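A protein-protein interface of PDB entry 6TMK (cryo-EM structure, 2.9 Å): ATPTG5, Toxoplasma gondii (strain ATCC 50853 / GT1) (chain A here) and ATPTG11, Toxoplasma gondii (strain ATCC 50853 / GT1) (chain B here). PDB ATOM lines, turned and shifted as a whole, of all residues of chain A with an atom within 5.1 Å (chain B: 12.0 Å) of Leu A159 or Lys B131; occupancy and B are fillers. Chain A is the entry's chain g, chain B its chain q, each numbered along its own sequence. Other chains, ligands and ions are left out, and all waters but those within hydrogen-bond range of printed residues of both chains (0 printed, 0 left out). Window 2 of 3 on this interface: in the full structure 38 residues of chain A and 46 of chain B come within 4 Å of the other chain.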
ATOM      1  N   HIS A 152      27.968   6.147  24.674  1.00  0.00           N
ATOM      2  CA  HIS A 152      27.671   6.827  23.421  1.00  0.00           C
ATOM      3  C   HIS A 152      26.184   6.771  23.099  1.00  0.00           C
ATOM      4  O   HIS A 152      25.526   7.806  22.941  1.00  0.00           O
ATOM      5  CB  HIS A 152      28.500   6.201  22.302  1.00  0.00           C
ATOM      6  CG  HIS A 152      28.096   6.641  20.933  1.00  0.00           C
ATOM      7  ND1 HIS A 152      28.109   7.961  20.542  1.00  0.00           N
ATOM      8  CD2 HIS A 152      27.679   5.934  19.859  1.00  0.00           C
ATOM      9  CE1 HIS A 152      27.708   8.048  19.288  1.00  0.00           C
ATOM     10  NE2 HIS A 152      27.440   6.832  18.850  1.00  0.00           N
ATOM     11  N   PRO A 154      23.567   5.505  24.998  1.00  0.00           N
ATOM     12  CA  PRO A 154      22.723   6.069  26.062  1.00  0.00           C
ATOM     13  C   PRO A 154      22.655   7.584  26.037  1.00  0.00           C
ATOM     14  O   PRO A 154      21.567   8.159  26.159  1.00  0.00           O
ATOM     15  CB  PRO A 154      23.395   5.548  27.333  1.00  0.00           C
ATOM     16  CG  PRO A 154      24.055   4.312  26.938  1.00  0.00           C
ATOM     17  CD  PRO A 154      24.463   4.457  25.512  1.00  0.00           C
ATOM     18  N   ARG A 155      23.800   8.250  25.896  1.00  0.00           N
ATOM     19  CA  ARG A 155      23.823   9.705  25.820  1.00  0.00           C
ATOM     20  C   ARG A 155      23.045  10.213  24.615  1.00  0.00           C
ATOM     21  O   ARG A 155      22.280  11.178  24.715  1.00  0.00           O
ATOM     22  CB  ARG A 155      25.268  10.174  25.759  1.00  0.00           C
ATOM     23  CG  ARG A 155      25.455  11.647  25.552  1.00  0.00           C
ATOM     24  CD  ARG A 155      26.851  12.028  25.930  1.00  0.00           C
ATOM     25  NE  ARG A 155      27.819  11.085  25.381  1.00  0.00           N
ATOM     26  CZ  ARG A 155      28.893  10.636  26.020  1.00  0.00           C
ATOM     27  NH1 ARG A 155      29.170  11.036  27.248  1.00  0.00           N
ATOM     28  NH2 ARG A 155      29.698   9.781  25.416  1.00  0.00           N
ATOM     29  N   GLN A 156      23.254   9.588  23.455  1.00  0.00           N
ATOM     30  CA  GLN A 156      22.529   9.971  22.250  1.00  0.00           C
ATOM     31  C   GLN A 156      21.023   9.871  22.459  1.00  0.00           C
ATOM     32  O   GLN A 156      20.270  10.796  22.127  1.00  0.00           O
ATOM     33  CB  GLN A 156      22.990   9.082  21.098  1.00  0.00           C
ATOM     34  CG  GLN A 156      22.686   9.594  19.718  1.00  0.00           C
ATOM     35  CD  GLN A 156      23.495   8.867  18.669  1.00  0.00           C
ATOM     36  OE1 GLN A 156      23.962   7.754  18.897  1.00  0.00           O
ATOM     37  NE2 GLN A 156      23.679   9.497  17.518  1.00  0.00           N
ATOM     38  N   MET A 157      20.568   8.749  23.020  1.00  0.00           N
ATOM     39  CA  MET A 157      19.144   8.558  23.258  1.00  0.00           C
ATOM     40  C   MET A 157      18.611   9.588  24.235  1.00  0.00           C
ATOM     41  O   MET A 157      17.525  10.139  24.037  1.00  0.00           O
ATOM     42  CB  MET A 157      18.878   7.147  23.771  1.00  0.00           C
ATOM     43  CG  MET A 157      17.416   6.849  24.036  1.00  0.00           C
ATOM     44  SD  MET A 157      16.354   7.065  22.603  1.00  0.00           S
ATOM     45  CE  MET A 157      17.011   5.800  21.538  1.00  0.00           C
ATOM     46  N   LEU A 158      19.353   9.847  25.307  1.00  0.00           N
ATOM     47  CA  LEU A 158      18.904  10.806  26.302  1.00  0.00           C
ATOM     48  C   LEU A 158      18.755  12.187  25.686  1.00  0.00           C
ATOM     49  O   LEU A 158      17.744  12.868  25.890  1.00  0.00           O
ATOM     50  CB  LEU A 158      19.890  10.839  27.463  1.00  0.00           C
ATOM     51  CG  LEU A 158      19.539  11.762  28.617  1.00  0.00           C
ATOM     52  CD1 LEU A 158      18.318  11.253  29.325  1.00  0.00           C
ATOM     53  CD2 LEU A 158      20.694  11.839  29.560  1.00  0.00           C
ATOM     54  N   LEU A 159      19.752  12.609  24.914  1.00  0.00           N
ATOM     55  CA  LEU A 159      19.700  13.925  24.294  1.00  0.00           C
ATOM     56  C   LEU A 159      18.542  14.028  23.314  1.00  0.00           C
ATOM     57  O   LEU A 159      17.834  15.041  23.287  1.00  0.00           O
ATOM     58  CB  LEU A 159      21.018  14.211  23.586  1.00  0.00           C
ATOM     59  CG  LEU A 159      22.242  14.303  24.488  1.00  0.00           C
ATOM     60  CD1 LEU A 159      23.503  14.189  23.666  1.00  0.00           C
ATOM     61  CD2 LEU A 159      22.236  15.584  25.266  1.00  0.00           C
ATOM     62  N   CYS A 160      18.324  12.995  22.501  1.00  0.00           N
ATOM     63  CA  CYS A 160      17.250  13.078  21.518  1.00  0.00           C
ATOM     64  C   CYS A 160      15.878  13.047  22.183  1.00  0.00           C
ATOM     65  O   CYS A 160      14.979  13.807  21.799  1.00  0.00           O
ATOM     66  CB  CYS A 160      17.381  11.949  20.502  1.00  0.00           C
ATOM     67  SG  CYS A 160      18.727  12.161  19.324  1.00  0.00           S
ATOM     68  N   ARG A 161      15.695  12.193  23.191  1.00  0.00           N
ATOM     69  CA  ARG A 161      14.424  12.168  23.899  1.00  0.00           C
ATOM     70  C   ARG A 161      14.180  13.460  24.661  1.00  0.00           C
ATOM     71  O   ARG A 161      13.024  13.849  24.858  1.00  0.00           O
ATOM     72  CB  ARG A 161      14.375  10.982  24.857  1.00  0.00           C
ATOM     73  CG  ARG A 161      14.377   9.619  24.195  1.00  0.00           C
ATOM     74  CD  ARG A 161      13.252   9.456  23.201  1.00  0.00           C
ATOM     75  NE  ARG A 161      11.945   9.681  23.804  1.00  0.00           N
ATOM     76  CZ  ARG A 161      11.264   8.762  24.474  1.00  0.00           C
ATOM     77  NH1 ARG A 161      11.764   7.545  24.639  1.00  0.00           N
ATOM     78  NH2 ARG A 161      10.083   9.064  24.987  1.00  0.00           N
ATOM     79  N   GLY A 162      15.240  14.136  25.105  1.00  0.00           N
ATOM     80  CA  GLY A 162      15.058  15.441  25.704  1.00  0.00           C
ATOM     81  C   GLY A 162      14.723  16.507  24.687  1.00  0.00           C
ATOM     82  O   GLY A 162      13.972  17.439  24.985  1.00  0.00           O
ATOM     83  N   ALA A 163      15.276  16.393  23.480  1.00  0.00           N
ATOM     84  CA  ALA A 163      14.888  17.298  22.407  1.00  0.00           C
ATOM     85  C   ALA A 163      13.417  17.124  22.059  1.00  0.00           C
ATOM     86  O   ALA A 163      12.730  18.096  21.729  1.00  0.00           O
ATOM     87  CB  ALA A 163      15.763  17.061  21.182  1.00  0.00           C
ATOM     88  N   ASP A 177      29.783   5.550  17.122  1.00  0.00           N
ATOM     89  CA  ASP A 177      30.732   6.537  17.614  1.00  0.00           C
ATOM     90  C   ASP A 177      31.904   6.690  16.659  1.00  0.00           C
ATOM     91  O   ASP A 177      32.489   5.701  16.208  1.00  0.00           O
ATOM     92  CB  ASP A 177      31.239   6.136  18.997  1.00  0.00           C
ATOM     93  CG  ASP A 177      31.794   7.307  19.775  1.00  0.00           C
ATOM     94  OD1 ASP A 177      31.738   8.444  19.264  1.00  0.00           O
ATOM     95  OD2 ASP A 177      32.290   7.089  20.899  1.00  0.00           O
ATOM     96  N   ALA A 178      32.241   7.938  16.351  1.00  0.00           N
ATOM     97  CA  ALA A 178      33.483   8.249  15.666  1.00  0.00           C
ATOM     98  C   ALA A 178      34.649   8.425  16.623  1.00  0.00           C
ATOM     99  O   ALA A 178      35.805   8.319  16.199  1.00  0.00           O
ATOM    100  CB  ALA A 178      33.314   9.519  14.834  1.00  0.00           C
ATOM    101  N   ARG A 179      34.375   8.694  17.900  1.00  0.00           N
ATOM    102  CA  ARG A 179      35.417   8.825  18.915  1.00  0.00           C
ATOM    103  C   ARG A 179      35.850   7.440  19.394  1.00  0.00           C
ATOM    104  O   ARG A 179      35.598   7.018  20.525  1.00  0.00           O
ATOM    105  CB  ARG A 179      34.926   9.681  20.070  1.00  0.00           C
ATOM    106  CG  ARG A 179      34.948  11.146  19.779  1.00  0.00           C
ATOM    107  CD  ARG A 179      34.689  11.963  21.015  1.00  0.00           C
ATOM    108  NE  ARG A 179      35.854  11.982  21.893  1.00  0.00           N
ATOM    109  CZ  ARG A 179      35.998  11.245  22.988  1.00  0.00           C
ATOM    110  NH1 ARG A 179      35.055  10.406  23.375  1.00  0.00           N
ATOM    111  NH2 ARG A 179      37.102  11.349  23.699  1.00  0.00           N
ATOM    112  N   ARG B 124      44.582  11.892  16.231  1.00  0.00           N
ATOM    113  CA  ARG B 124      44.111  12.309  17.542  1.00  0.00           C
ATOM    114  C   ARG B 124      42.600  12.153  17.599  1.00  0.00           C
ATOM    115  O   ARG B 124      41.892  12.540  16.665  1.00  0.00           O
ATOM    116  CB  ARG B 124      44.501  13.758  17.844  1.00  0.00           C
ATOM    117  CG  ARG B 124      44.264  14.163  19.281  1.00  0.00           C
ATOM    118  CD  ARG B 124      44.595  15.620  19.513  1.00  0.00           C
ATOM    119  NE  ARG B 124      46.023  15.812  19.743  1.00  0.00           N
ATOM    120  CZ  ARG B 124      46.603  16.995  19.913  1.00  0.00           C
ATOM    121  NH1 ARG B 124      45.882  18.106  19.878  1.00  0.00           N
ATOM    122  NH2 ARG B 124      47.910  17.065  20.117  1.00  0.00           N
ATOM    123  N   VAL B 125      42.114  11.594  18.697  1.00  0.00           N
ATOM    124  CA  VAL B 125      40.669  11.391  18.843  1.00  0.00           C
ATOM    125  C   VAL B 125      39.986  12.748  18.958  1.00  0.00           C
ATOM    126  O   VAL B 125      40.533  13.655  19.609  1.00  0.00           O
ATOM    127  CB  VAL B 125      40.379  10.519  20.065  1.00  0.00           C
ATOM    128  CG1 VAL B 125      38.897  10.269  20.205  1.00  0.00           C
ATOM    129  CG2 VAL B 125      41.122   9.210  19.959  1.00  0.00           C
ATOM    130  N   PRO B 126      38.804  12.943  18.366  1.00  0.00           N
ATOM    131  CA  PRO B 126      38.124  14.236  18.507  1.00  0.00           C
ATOM    132  C   PRO B 126      37.736  14.545  19.942  1.00  0.00           C
ATOM    133  O   PRO B 126      37.910  13.716  20.838  1.00  0.00           O
ATOM    134  CB  PRO B 126      36.886  14.083  17.616  1.00  0.00           C
ATOM    135  CG  PRO B 126      37.222  13.002  16.679  1.00  0.00           C
ATOM    136  CD  PRO B 126      38.093  12.061  17.429  1.00  0.00           C
ATOM    137  N   SER B 127      37.206  15.741  20.162  1.00  0.00           N
ATOM    138  CA  SER B 127      36.822  16.159  21.499  1.00  0.00           C
ATOM    139  C   SER B 127      35.466  15.581  21.871  1.00  0.00           C
ATOM    140  O   SER B 127      34.601  15.359  21.019  1.00  0.00           O
ATOM    141  CB  SER B 127      36.782  17.680  21.599  1.00  0.00           C
ATOM    142  OG  SER B 127      36.094  18.088  22.765  1.00  0.00           O
ATOM    143  N   ILE B 128      35.291  15.333  23.169  1.00  0.00           N
ATOM    144  CA  ILE B 128      34.062  14.738  23.671  1.00  0.00           C
ATOM    145  C   ILE B 128      32.876  15.685  23.616  1.00  0.00           C
ATOM    146  O   ILE B 128      31.740  15.250  23.825  1.00  0.00           O
ATOM    147  CB  ILE B 128      34.305  14.244  25.111  1.00  0.00           C
ATOM    148  CG1 ILE B 128      33.136  13.392  25.592  1.00  0.00           C
ATOM    149  CG2 ILE B 128      34.542  15.411  26.041  1.00  0.00           C
ATOM    150  CD1 ILE B 128      33.509  12.471  26.715  1.00  0.00           C
ATOM    151  N   LEU B 129      33.108  16.968  23.347  1.00  0.00           N
ATOM    152  CA  LEU B 129      32.020  17.931  23.248  1.00  0.00           C
ATOM    153  C   LEU B 129      31.268  17.834  21.931  1.00  0.00           C
ATOM    154  O   LEU B 129      30.133  18.316  21.836  1.00  0.00           O
ATOM    155  CB  LEU B 129      32.569  19.343  23.418  1.00  0.00           C
ATOM    156  CG  LEU B 129      33.290  19.610  24.733  1.00  0.00           C
ATOM    157  CD1 LEU B 129      34.257  20.754  24.580  1.00  0.00           C
ATOM    158  CD2 LEU B 129      32.290  19.920  25.822  1.00  0.00           C
ATOM    159  N   THR B 130      31.868  17.219  20.914  1.00  0.00           N
ATOM    160  CA  THR B 130      31.157  16.976  19.669  1.00  0.00           C
ATOM    161  C   THR B 130      29.973  16.047  19.867  1.00  0.00           C
ATOM    162  O   THR B 130      29.057  16.039  19.037  1.00  0.00           O
ATOM    163  CB  THR B 130      32.112  16.388  18.639  1.00  0.00           C
ATOM    164  OG1 THR B 130      32.641  15.152  19.128  1.00  0.00           O
ATOM    165  CG2 THR B 130      33.255  17.342  18.390  1.00  0.00           C
ATOM    166  N   LYS B 131      29.973  15.264  20.943  1.00  0.00           N
ATOM    167  CA  LYS B 131      28.821  14.433  21.257  1.00  0.00           C
ATOM    168  C   LYS B 131      27.604  15.285  21.579  1.00  0.00           C
ATOM    169  O   LYS B 131      26.483  14.963  21.172  1.00  0.00           O
ATOM    170  CB  LYS B 131      29.167  13.509  22.419  1.00  0.00           C
ATOM    171  CG  LYS B 131      30.344  12.591  22.130  1.00  0.00           C
ATOM    172  CD  LYS B 131      30.006  11.471  21.158  1.00  0.00           C
ATOM    173  CE  LYS B 131      30.448  11.810  19.745  1.00  0.00           C
ATOM    174  NZ  LYS B 131      30.252  10.684  18.803  1.00  0.00           N
ATOM    175  N   TYR B 132      27.805  16.372  22.316  1.00  0.00           N
ATOM    176  CA  TYR B 132      26.754  17.335  22.599  1.00  0.00           C
ATOM    177  C   TYR B 132      26.664  18.428  21.546  1.00  0.00           C
ATOM    178  O   TYR B 132      25.820  19.321  21.670  1.00  0.00           O
ATOM    179  CB  TYR B 132      26.986  17.967  23.967  1.00  0.00           C
ATOM    180  CG  TYR B 132      27.236  16.978  25.074  1.00  0.00           C
ATOM    181  CD1 TYR B 132      26.195  16.481  25.834  1.00  0.00           C
ATOM    182  CD2 TYR B 132      28.514  16.541  25.359  1.00  0.00           C
ATOM    183  CE1 TYR B 132      26.421  15.586  26.845  1.00  0.00           C
ATOM    184  CE2 TYR B 132      28.747  15.642  26.366  1.00  0.00           C
ATOM    185  CZ  TYR B 132      27.697  15.165  27.104  1.00  0.00           C
ATOM    186  OH  TYR B 132      27.918  14.266  28.114  1.00  0.00           O
ATOM    187  N   HIS B 133      27.509  18.378  20.520  1.00  0.00           N
ATOM    188  CA  HIS B 133      27.451  19.315  19.401  1.00  0.00           C
ATOM    189  C   HIS B 133      27.731  20.746  19.861  1.00  0.00           C
ATOM    190  O   HIS B 133      26.885  21.639  19.769  1.00  0.00           O
ATOM    191  CB  HIS B 133      26.098  19.215  18.697  1.00  0.00           C
ATOM    192  CG  HIS B 133      25.735  17.818  18.305  1.00  0.00           C
ATOM    193  ND1 HIS B 133      26.481  17.079  17.413  1.00  0.00           N
ATOM    194  CD2 HIS B 133      24.712  17.022  18.692  1.00  0.00           C
ATOM    195  CE1 HIS B 133      25.930  15.888  17.263  1.00  0.00           C
ATOM    196  NE2 HIS B 133      24.856  15.827  18.029  1.00  0.00           N
ATOM    197  N   LEU B 134      28.945  20.949  20.361  1.00  0.00           N
ATOM    198  CA  LEU B 134      29.365  22.252  20.858  1.00  0.00           C
ATOM    199  C   LEU B 134      30.642  22.691  20.152  1.00  0.00           C
ATOM    200  O   LEU B 134      31.646  21.979  20.173  1.00  0.00           O
ATOM    201  CB  LEU B 134      29.584  22.217  22.371  1.00  0.00           C
ATOM    202  CG  LEU B 134      28.538  21.452  23.174  1.00  0.00           C
ATOM    203  CD1 LEU B 134      29.020  21.237  24.590  1.00  0.00           C
ATOM    204  CD2 LEU B 134      27.236  22.205  23.159  1.00  0.00           C
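Of chain A, only His A152 (3.7 Å), Leu A159 (3.96 Å) and Asp A177 (2.7 Å) come within 4 Å of Lys B131.
His A152 touches one residue of chain B.
Arg A155 touches just one residue of chain B: Tyr B132.
No residue of chain B comes within 4 Å of Gln A156.
No residue of chain B comes within 4 Å of Cys A160.
Of the printed residues of chain A, Ser B127 touches Arg A179.
Printed residues of chain A within 4 Å of Pro B126: Arg A179 (2.9 Å).
The nearest printed residue of chain A that does not touch Tyr B132 is Leu A159 (4.1 Å).
The backbone carbonyl oxygen of Pro B126 lies within hydrogen-bond range of the guanidinium group of Arg A179 (2.9 Å).
NZ of Lys B131 lies within salt-bridge range of OD1 of Asp A177.
Among the printed residues, merely in contact across the chains: His A152 with Lys B131 (3.7 Å), Arg A155 with Tyr B132 (3.3 Å), Leu A159 with Lys B131 (3.96 Å), Arg A179 with Val B125 (3.9 Å), Arg A179 with Ser B127 (3.4 Å) and Arg A179 with Ile B128 (3.6 Å).
Of the 11 printed residues of chain B, 6 touch a printed residue of chain A.
Hydrophobic or aromatic side chains of chain B that line the printed part of chain A: Val B125 and Tyr B132.
Of the 14 printed residues of chain A, 5 touch a printed residue of chain B.
Hydrophobic or aromatic side chains of chain A that line the printed part of chain B: His A152 and Leu A159.
Among the printed residues, 8 pairs touch across the chains.
Among the printed residues, Asp or Glu carboxylates within 4 Å of a Lys or Arg side-chain nitrogen of the other chain: Asp A177 with Lys B131 (2.7 Å).
N of Leu B129 lies close to OG of Ser B127.
O of Ser B127 lies within hydrogen-bond range of OG1 of Thr B130 (2.7 Å).
A ring nitrogen (NE2) of His A152 is in hydrogen-bond range of the backbone NH (N) of Asp A177.
The side-chain carboxylate (OD1) of Asp A177 sits at hydrogen-bond distance from the backbone NH (N) of Arg A179 (3.0 Å).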
